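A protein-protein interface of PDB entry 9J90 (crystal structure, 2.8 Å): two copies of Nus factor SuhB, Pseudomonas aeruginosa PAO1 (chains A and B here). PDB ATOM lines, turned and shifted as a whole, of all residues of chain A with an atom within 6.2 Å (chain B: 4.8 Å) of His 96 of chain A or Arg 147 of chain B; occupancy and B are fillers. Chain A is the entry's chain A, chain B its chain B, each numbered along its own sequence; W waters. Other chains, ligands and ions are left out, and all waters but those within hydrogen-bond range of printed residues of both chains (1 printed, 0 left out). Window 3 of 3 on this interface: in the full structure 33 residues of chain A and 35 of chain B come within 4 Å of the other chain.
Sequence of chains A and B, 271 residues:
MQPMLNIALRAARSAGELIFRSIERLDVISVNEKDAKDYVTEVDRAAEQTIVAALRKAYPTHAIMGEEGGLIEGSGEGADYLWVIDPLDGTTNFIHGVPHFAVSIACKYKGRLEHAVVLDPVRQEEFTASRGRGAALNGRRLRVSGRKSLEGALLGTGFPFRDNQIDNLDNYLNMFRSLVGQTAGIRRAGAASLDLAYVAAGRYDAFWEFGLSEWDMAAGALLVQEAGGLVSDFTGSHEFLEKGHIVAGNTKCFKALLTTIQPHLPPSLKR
NE of Arg 203 of chain B lies within hydrogen-bond range of O of Gly 97 of chain A, 3.2 Å away.
The guanidinium group of Arg 147 of chain B is in hydrogen-bond range of a ring nitrogen (NE2) of His 96 of chain A, at 3.3 Å.
The side-chain carboxylate (OE2) of Glu 33 of chain A is in hydrogen-bond range of the backbone NH (N) of Lys 148 of chain B.
The side-chain carboxylate (OD2) of Asp 205 of chain B is in hydrogen-bond range of a ring nitrogen (NE2) of His 96 of chain A (3.2 Å).
His 96 of chain A touches just these residues of chain B: Arg 147 (3.3 Å), Gly 152 (3.8 Å), Leu 154 (3.5 Å), Gly 202 (3.6 Å), Arg 203 (3.2 Å) and Asp 205 (3.2 Å).
Printed residues of chain B within 4 Å of Gly 97 of chain A: Arg 203 (3.2 Å).
Ser 145 of chain B touches none of the printed residues of chain A.
Arg 147 of chain B touches two residues of chain A.
Printed residues of chain A within 4 Å of Gly 152 of chain B: His 96.
Ala 153 of chain B touches none of the printed residues of chain A.
Printed residues of chain A within 4 Å of Asp 205 of chain B: His 96 (3.2 Å).
The nearest residue of chain B that does not touch His 96 of chain A is Ala 153 of chain B (4.4 Å).
The nearest residue of chain A that does not touch Arg 147 of chain B is Ala 36 of chain A (5.2 Å).
Glu 33 of chain A touches Arg 147 of chain B (OE2 to CA, 3.2 Å).
His 96 of chain A touches Gly 152 of chain B (CE1 to O, 3.8 Å).
His 96 of chain A touches Leu 154 of chain B.
His 96 of chain A touches Gly 202 of chain B.
Arg 203 of chain B touches His 96 of chain A.
Leu 154 of chain B touches Val 98 of chain A (CD2 to CG2, 3.8 Å).
Arg 203 of chain B touches Val 98 of chain A (O to CG2, 3.5 Å).
Water W1 lies within hydrogen-bond range of NH1 of Arg 147 of chain B (2.5 Å), OD1 of Asp 205 of chain B (3.0 Å) and NE2 of His 96 of chain A (3.4 Å).
The backbone carbonyl oxygen of Asn 93 of chain A lies within hydrogen-bond range of the backbone NH of Val 98 of chain A, at 2.8 Å.
The backbone carbonyl oxygen (O) of Asp 205 of chain B lies within hydrogen-bond range of the backbone NH (N) of Asn 250 of chain B.
NZ of Lys 148 of chain B is in hydrogen-bond range of O of Gly 146 of chain B (3.3 Å).
The guanidinium group (NH1) of Arg 147 of chain B lies within salt-bridge range of the side-chain carboxylate (OD2) of Asp 205 of chain B.
The side-chain hydroxyl (OG) of Ser 145 of chain B sits at hydrogen-bond distance from the side-chain carboxylate (OD1) of Asp 205 of chain B, at 2.6 Å.
The backbone carbonyl oxygen (O) of Thr 92 of chain A lies within hydrogen-bond range of a ring nitrogen (ND1) of His 96 of chain A, 2.9 Å away.
No position is printed for both chains.
Of the 15 printed residues of chain B, 7 touch a printed residue of chain A.
Along chain B the printed residues that touch a printed residue of chain A span positions 147 to 205.
Of the 14 printed residues of chain A, 4 touch a printed residue of chain B.
Among the printed residues, 11 pairs touch across the chains.
Among the printed residues, no Asp or Glu carboxylate lies within 4 Å of a Lys or Arg side-chain nitrogen of the other chain.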
ATOM      1  N   ILE A  23     -22.695  11.033  20.301  1.00  0.00           N
ATOM      2  CA  ILE A  23     -23.121  12.344  19.751  1.00  0.00           C
ATOM      3  C   ILE A  23     -22.636  13.471  20.665  1.00  0.00           C
ATOM      4  O   ILE A  23     -22.178  14.502  20.157  1.00  0.00           O
ATOM      5  CB  ILE A  23     -24.649  12.395  19.492  1.00  0.00           C
ATOM      6  CG1 ILE A  23     -25.025  13.618  18.649  1.00  0.00           C
ATOM      7  CG2 ILE A  23     -25.465  12.335  20.775  1.00  0.00           C
ATOM      8  CD1 ILE A  23     -25.647  13.300  17.311  1.00  0.00           C
ATOM      9  N   LEU A  26     -18.969  14.002  19.859  1.00  0.00           N
ATOM     10  CA  LEU A  26     -18.993  14.590  18.493  1.00  0.00           C
ATOM     11  C   LEU A  26     -19.174  16.105  18.554  1.00  0.00           C
ATOM     12  O   LEU A  26     -18.433  16.816  17.873  1.00  0.00           O
ATOM     13  CB  LEU A  26     -20.153  13.964  17.707  1.00  0.00           C
ATOM     14  CG  LEU A  26     -20.117  14.220  16.206  1.00  0.00           C
ATOM     15  CD1 LEU A  26     -20.902  13.150  15.469  1.00  0.00           C
ATOM     16  CD2 LEU A  26     -20.644  15.607  15.856  1.00  0.00           C
ATOM     17  N   ASP A  27     -20.175  16.548  19.313  1.00  0.00           N
ATOM     18  CA  ASP A  27     -20.726  17.932  19.244  1.00  0.00           C
ATOM     19  C   ASP A  27     -19.681  18.935  19.764  1.00  0.00           C
ATOM     20  O   ASP A  27     -19.680  20.085  19.262  1.00  0.00           O
ATOM     21  CB  ASP A  27     -22.123  18.079  19.884  1.00  0.00           C
ATOM     22  CG  ASP A  27     -23.295  18.050  18.892  1.00  0.00           C
ATOM     23  OD1 ASP A  27     -23.630  19.121  18.290  1.00  0.00           O
ATOM     24  OD2 ASP A  27     -23.876  16.960  18.716  1.00  0.00           O
ATOM     25  N   ASN A  32     -13.890  15.911  10.765  1.00  0.00           N
ATOM     26  CA  ASN A  32     -13.870  16.593   9.439  1.00  0.00           C
ATOM     27  C   ASN A  32     -14.287  15.594   8.359  1.00  0.00           C
ATOM     28  O   ASN A  32     -14.584  14.470   8.718  1.00  0.00           O
ATOM     29  CB  ASN A  32     -12.504  17.217   9.143  1.00  0.00           C
ATOM     30  CG  ASN A  32     -11.419  16.207   8.833  1.00  0.00           C
ATOM     31  OD1 ASN A  32     -11.706  15.107   8.385  1.00  0.00           O
ATOM     32  ND2 ASN A  32     -10.169  16.559   9.082  1.00  0.00           N
ATOM     33  N   GLU A  33     -14.329  16.009   7.092  1.00  0.00           N
ATOM     34  CA  GLU A  33     -14.933  15.247   5.962  1.00  0.00           C
ATOM     35  C   GLU A  33     -14.461  13.791   5.932  1.00  0.00           C
ATOM     36  O   GLU A  33     -15.316  12.907   5.985  1.00  0.00           O
ATOM     37  CB  GLU A  33     -14.574  15.924   4.644  1.00  0.00           C
ATOM     38  CG  GLU A  33     -15.343  17.200   4.438  1.00  0.00           C
ATOM     39  CD  GLU A  33     -14.607  18.280   3.675  1.00  0.00           C
ATOM     40  OE1 GLU A  33     -13.751  17.940   2.841  1.00  0.00           O
ATOM     41  OE2 GLU A  33     -14.905  19.462   3.915  1.00  0.00           O
ATOM     42  N   ALA A  36     -15.474  11.217   8.673  1.00  0.00           N
ATOM     43  CA  ALA A  36     -16.913  11.120   9.016  1.00  0.00           C
ATOM     44  C   ALA A  36     -17.421   9.697   8.817  1.00  0.00           C
ATOM     45  O   ALA A  36     -18.103   9.146   9.700  1.00  0.00           O
ATOM     46  CB  ALA A  36     -17.697  12.108   8.207  1.00  0.00           C
ATOM     47  N   THR A  91     -27.836   7.968   9.918  1.00  0.00           N
ATOM     48  CA  THR A  91     -26.380   8.116  10.149  1.00  0.00           C
ATOM     49  C   THR A  91     -25.893   9.491   9.683  1.00  0.00           C
ATOM     50  O   THR A  91     -24.954  10.044  10.274  1.00  0.00           O
ATOM     51  CB  THR A  91     -25.652   6.945   9.476  1.00  0.00           C
ATOM     52  OG1 THR A  91     -25.971   7.018   8.095  1.00  0.00           O
ATOM     53  CG2 THR A  91     -26.071   5.571   9.946  1.00  0.00           C
ATOM     54  N   THR A  92     -26.459  10.005   8.593  1.00  0.00           N
ATOM     55  CA  THR A  92     -26.061  11.339   8.100  1.00  0.00           C
ATOM     56  C   THR A  92     -26.420  12.419   9.117  1.00  0.00           C
ATOM     57  O   THR A  92     -25.585  13.269   9.450  1.00  0.00           O
ATOM     58  CB  THR A  92     -26.683  11.647   6.743  1.00  0.00           C
ATOM     59  OG1 THR A  92     -26.048  10.743   5.857  1.00  0.00           O
ATOM     60  CG2 THR A  92     -26.421  13.058   6.285  1.00  0.00           C
ATOM     61  N   ASN A  93     -27.653  12.375   9.598  1.00  0.00           N
ATOM     62  CA  ASN A  93     -28.086  13.203  10.736  1.00  0.00           C
ATOM     63  C   ASN A  93     -27.112  13.037  11.894  1.00  0.00           C
ATOM     64  O   ASN A  93     -26.577  14.028  12.407  1.00  0.00           O
ATOM     65  CB  ASN A  93     -29.486  12.800  11.198  1.00  0.00           C
ATOM     66  CG  ASN A  93     -30.573  13.169  10.211  1.00  0.00           C
ATOM     67  OD1 ASN A  93     -30.320  13.899   9.285  1.00  0.00           O
ATOM     68  ND2 ASN A  93     -31.789  12.705  10.411  1.00  0.00           N
ATOM     69  N   PHE A  94     -26.874  11.799  12.290  1.00  0.00           N
ATOM     70  CA  PHE A  94     -26.017  11.529  13.468  1.00  0.00           C
ATOM     71  C   PHE A  94     -24.673  12.212  13.308  1.00  0.00           C
ATOM     72  O   PHE A  94     -24.256  12.986  14.170  1.00  0.00           O
ATOM     73  CB  PHE A  94     -25.805  10.025  13.686  1.00  0.00           C
ATOM     74  CG  PHE A  94     -24.760   9.754  14.739  1.00  0.00           C
ATOM     75  CD1 PHE A  94     -25.083   9.798  16.091  1.00  0.00           C
ATOM     76  CD2 PHE A  94     -23.432   9.548  14.387  1.00  0.00           C
ATOM     77  CE1 PHE A  94     -24.115   9.606  17.070  1.00  0.00           C
ATOM     78  CE2 PHE A  94     -22.462   9.382  15.362  1.00  0.00           C
ATOM     79  CZ  PHE A  94     -22.802   9.398  16.702  1.00  0.00           C
ATOM     80  N   ILE A  95     -23.990  11.925  12.217  1.00  0.00           N
ATOM     81  CA  ILE A  95     -22.606  12.423  12.012  1.00  0.00           C
ATOM     82  C   ILE A  95     -22.615  13.945  11.891  1.00  0.00           C
ATOM     83  O   ILE A  95     -21.572  14.557  12.153  1.00  0.00           O
ATOM     84  CB  ILE A  95     -21.977  11.734  10.772  1.00  0.00           C
ATOM     85  CG1 ILE A  95     -20.449  11.824  10.739  1.00  0.00           C
ATOM     86  CG2 ILE A  95     -22.535  12.284   9.475  1.00  0.00           C
ATOM     87  CD1 ILE A  95     -19.743  11.358  11.998  1.00  0.00           C
ATOM     88  N   HIS A  96     -23.737  14.555  11.528  1.00  0.00           N
ATOM     89  CA  HIS A  96     -23.800  16.024  11.530  1.00  0.00           C
ATOM     90  C   HIS A  96     -24.249  16.599  12.862  1.00  0.00           C
ATOM     91  O   HIS A  96     -24.255  17.841  12.978  1.00  0.00           O
ATOM     92  CB  HIS A  96     -24.719  16.466  10.419  1.00  0.00           C
ATOM     93  CG  HIS A  96     -24.025  16.457   9.105  1.00  0.00           C
ATOM     94  ND1 HIS A  96     -23.751  15.296   8.416  1.00  0.00           N
ATOM     95  CD2 HIS A  96     -23.536  17.461   8.360  1.00  0.00           C
ATOM     96  CE1 HIS A  96     -23.164  15.590   7.286  1.00  0.00           C
ATOM     97  NE2 HIS A  96     -23.010  16.902   7.231  1.00  0.00           N
ATOM     98  N   GLY A  97     -24.667  15.756  13.803  1.00  0.00           N
ATOM     99  CA  GLY A  97     -25.210  16.209  15.084  1.00  0.00           C
ATOM    100  C   GLY A  97     -26.689  16.546  15.061  1.00  0.00           C
ATOM    101  O   GLY A  97     -27.190  17.068  16.060  1.00  0.00           O
ATOM    102  N   VAL A  98     -27.396  16.241  13.985  1.00  0.00           N
ATOM    103  CA  VAL A  98     -28.854  16.450  13.917  1.00  0.00           C
ATOM    104  C   VAL A  98     -29.531  15.434  14.828  1.00  0.00           C
ATOM    105  O   VAL A  98     -29.425  14.224  14.597  1.00  0.00           O
ATOM    106  CB  VAL A  98     -29.340  16.357  12.467  1.00  0.00           C
ATOM    107  CG1 VAL A  98     -30.854  16.254  12.404  1.00  0.00           C
ATOM    108  CG2 VAL A  98     -28.837  17.548  11.673  1.00  0.00           C
ATOM    109  N   SER B 145     -20.092  24.538  10.748  1.00  0.00           N
ATOM    110  CA  SER B 145     -19.304  23.355  10.371  1.00  0.00           C
ATOM    111  C   SER B 145     -18.073  23.786   9.589  1.00  0.00           C
ATOM    112  O   SER B 145     -18.042  24.937   9.049  1.00  0.00           O
ATOM    113  CB  SER B 145     -20.136  22.367   9.582  1.00  0.00           C
ATOM    114  OG  SER B 145     -20.379  22.813   8.266  1.00  0.00           O
ATOM    115  N   GLY B 146     -17.142  22.848   9.434  1.00  0.00           N
ATOM    116  CA  GLY B 146     -15.891  23.109   8.726  1.00  0.00           C
ATOM    117  C   GLY B 146     -15.877  22.560   7.319  1.00  0.00           C
ATOM    118  O   GLY B 146     -14.882  22.753   6.609  1.00  0.00           O
ATOM    119  N   ARG B 147     -16.902  21.848   6.907  1.00  0.00           N
ATOM    120  CA  ARG B 147     -16.932  21.222   5.570  1.00  0.00           C
ATOM    121  C   ARG B 147     -16.575  22.240   4.500  1.00  0.00           C
ATOM    122  O   ARG B 147     -17.113  23.357   4.473  1.00  0.00           O
ATOM    123  CB  ARG B 147     -18.314  20.615   5.332  1.00  0.00           C
ATOM    124  CG  ARG B 147     -18.567  20.252   3.886  1.00  0.00           C
ATOM    125  CD  ARG B 147     -19.738  19.314   3.749  1.00  0.00           C
ATOM    126  NE  ARG B 147     -19.265  17.954   3.917  1.00  0.00           N
ATOM    127  CZ  ARG B 147     -19.398  17.212   5.009  1.00  0.00           C
ATOM    128  NH1 ARG B 147     -20.040  17.668   6.077  1.00  0.00           N
ATOM    129  NH2 ARG B 147     -18.892  15.994   5.014  1.00  0.00           N
ATOM    130  N   LYS B 148     -15.733  21.824   3.566  1.00  0.00           N
ATOM    131  CA  LYS B 148     -15.086  22.747   2.601  1.00  0.00           C
ATOM    132  C   LYS B 148     -15.884  22.817   1.297  1.00  0.00           C
ATOM    133  O   LYS B 148     -15.600  23.701   0.469  1.00  0.00           O
ATOM    134  CB  LYS B 148     -13.612  22.344   2.435  1.00  0.00           C
ATOM    135  CG  LYS B 148     -12.691  22.860   3.545  1.00  0.00           C
ATOM    136  CD  LYS B 148     -12.526  24.390   3.553  1.00  0.00           C
ATOM    137  CE  LYS B 148     -11.762  24.951   4.735  1.00  0.00           C
ATOM    138  NZ  LYS B 148     -12.633  25.042   5.933  1.00  0.00           N
ATOM    139  N   SER B 149     -16.825  21.911   1.085  1.00  0.00           N
ATOM    140  CA  SER B 149     -17.542  21.825  -0.195  1.00  0.00           C
ATOM    141  C   SER B 149     -18.882  21.133   0.028  1.00  0.00           C
ATOM    142  O   SER B 149     -19.118  20.614   1.108  1.00  0.00           O
ATOM    143  CB  SER B 149     -16.725  21.087  -1.215  1.00  0.00           C
ATOM    144  OG  SER B 149     -17.012  19.686  -1.170  1.00  0.00           O
ATOM    145  N   GLU B 151     -19.643  18.367  -1.210  1.00  0.00           N
ATOM    146  CA  GLU B 151     -19.437  16.905  -1.174  1.00  0.00           C
ATOM    147  C   GLU B 151     -19.780  16.367   0.206  1.00  0.00           C
ATOM    148  O   GLU B 151     -19.111  16.730   1.177  1.00  0.00           O
ATOM    149  CB  GLU B 151     -17.995  16.452  -1.414  1.00  0.00           C
ATOM    150  CG  GLU B 151     -17.809  15.714  -2.705  1.00  0.00           C
ATOM    151  CD  GLU B 151     -18.446  14.341  -2.823  1.00  0.00           C
ATOM    152  OE1 GLU B 151     -17.953  13.440  -2.118  1.00  0.00           O
ATOM    153  OE2 GLU B 151     -19.400  14.164  -3.657  1.00  0.00           O
ATOM    154  N   GLY B 152     -20.790  15.523   0.281  1.00  0.00           N
ATOM    155  CA  GLY B 152     -21.235  14.980   1.567  1.00  0.00           C
ATOM    156  C   GLY B 152     -21.933  15.975   2.480  1.00  0.00           C
ATOM    157  O   GLY B 152     -22.151  15.664   3.639  1.00  0.00           O
ATOM    158  N   ALA B 153     -22.294  17.147   1.973  1.00  0.00           N
ATOM    159  CA  ALA B 153     -22.968  18.170   2.792  1.00  0.00           C
ATOM    160  C   ALA B 153     -24.401  17.778   3.146  1.00  0.00           C
ATOM    161  O   ALA B 153     -25.066  17.108   2.384  1.00  0.00           O
ATOM    162  CB  ALA B 153     -22.967  19.478   2.059  1.00  0.00           C
ATOM    163  N   LEU B 154     -24.834  18.211   4.315  1.00  0.00           N
ATOM    164  CA  LEU B 154     -26.235  18.094   4.751  1.00  0.00           C
ATOM    165  C   LEU B 154     -26.850  19.473   4.702  1.00  0.00           C
ATOM    166  O   LEU B 154     -26.444  20.311   5.521  1.00  0.00           O
ATOM    167  CB  LEU B 154     -26.304  17.514   6.171  1.00  0.00           C
ATOM    168  CG  LEU B 154     -27.718  17.335   6.737  1.00  0.00           C
ATOM    169  CD1 LEU B 154     -28.567  16.437   5.840  1.00  0.00           C
ATOM    170  CD2 LEU B 154     -27.687  16.764   8.136  1.00  0.00           C
ATOM    171  N   GLY B 202     -23.616  23.934  13.382  1.00  0.00           N
ATOM    172  CA  GLY B 202     -22.861  23.002  12.544  1.00  0.00           C
ATOM    173  C   GLY B 202     -23.621  21.768  12.146  1.00  0.00           C
ATOM    174  O   GLY B 202     -22.998  20.904  11.482  1.00  0.00           O
ATOM    175  N   ARG B 203     -24.922  21.719  12.424  1.00  0.00           N
ATOM    176  CA  ARG B 203     -25.753  20.529  12.145  1.00  0.00           C
ATOM    177  C   ARG B 203     -26.178  20.489  10.693  1.00  0.00           C
ATOM    178  O   ARG B 203     -26.317  19.387  10.147  1.00  0.00           O
ATOM    179  CB  ARG B 203     -26.957  20.502  13.087  1.00  0.00           C
ATOM    180  CG  ARG B 203     -26.593  20.209  14.532  1.00  0.00           C
ATOM    181  CD  ARG B 203     -27.688  20.617  15.457  1.00  0.00           C
ATOM    182  NE  ARG B 203     -27.483  20.172  16.823  1.00  0.00           N
ATOM    183  CZ  ARG B 203     -28.393  20.288  17.789  1.00  0.00           C
ATOM    184  NH1 ARG B 203     -29.585  20.797  17.527  1.00  0.00           N
ATOM    185  NH2 ARG B 203     -28.117  19.873  19.008  1.00  0.00           N
ATOM    186  N   ASP B 205     -24.859  22.191   6.983  1.00  0.00           N
ATOM    187  CA  ASP B 205     -23.739  22.942   6.384  1.00  0.00           C
ATOM    188  C   ASP B 205     -24.230  24.203   5.647  1.00  0.00           C
ATOM    189  O   ASP B 205     -23.440  25.150   5.502  1.00  0.00           O
ATOM    190  CB  ASP B 205     -22.897  22.035   5.490  1.00  0.00           C
ATOM    191  CG  ASP B 205     -22.426  20.794   6.211  1.00  0.00           C
ATOM    192  OD1 ASP B 205     -21.886  20.948   7.311  1.00  0.00           O
ATOM    193  OD2 ASP B 205     -22.607  19.684   5.673  1.00  0.00           O
ATOM    194  N   ASN B 250     -22.083  27.729   6.382  1.00  0.00           N
ATOM    195  CA  ASN B 250     -20.636  27.921   6.618  1.00  0.00           C
ATOM    196  C   ASN B 250     -20.087  28.661   5.406  1.00  0.00           C
ATOM    197  O   ASN B 250     -20.797  28.810   4.408  1.00  0.00           O
ATOM    198  CB  ASN B 250     -19.865  26.630   6.958  1.00  0.00           C
ATOM    199  CG  ASN B 250     -19.504  25.723   5.788  1.00  0.00           C
ATOM    200  OD1 ASN B 250     -19.449  26.140   4.616  1.00  0.00           O
ATOM    201  ND2 ASN B 250     -19.172  24.478   6.120  1.00  0.00           N
ATOM    202  N   LYS B 252     -17.774  28.196   2.876  1.00  0.00           N
ATOM    203  CA  LYS B 252     -17.662  27.554   1.561  1.00  0.00           C
ATOM    204  C   LYS B 252     -19.006  27.033   1.060  1.00  0.00           C
ATOM    205  O   LYS B 252     -19.333  27.155  -0.119  1.00  0.00           O
ATOM    206  CB  LYS B 252     -16.682  26.381   1.655  1.00  0.00           C
ATOM    207  CG  LYS B 252     -15.357  26.667   2.361  1.00  0.00           C
ATOM    208  CD  LYS B 252     -14.307  27.334   1.497  1.00  0.00           C
ATOM    209  CE  LYS B 252     -13.526  28.409   2.221  1.00  0.00           C
ATOM    210  NZ  LYS B 252     -12.900  29.338   1.248  1.00  0.00           N
ATOM    211  N   CYS B 253     -19.781  26.437   1.938  1.00  0.00           N
ATOM    212  CA  CYS B 253     -21.075  25.834   1.543  1.00  0.00           C
ATOM    213  C   CYS B 253     -22.121  26.933   1.308  1.00  0.00           C
ATOM    214  O   CYS B 253     -22.965  26.776   0.414  1.00  0.00           O
ATOM    215  CB  CYS B 253     -21.530  24.785   2.564  1.00  0.00           C
ATOM    216  SG  CYS B 253     -20.504  23.281   2.660  1.00  0.00           S
HETATM  217  O   HOH W   1     -20.282  18.603   8.341  1.00  0.00           O
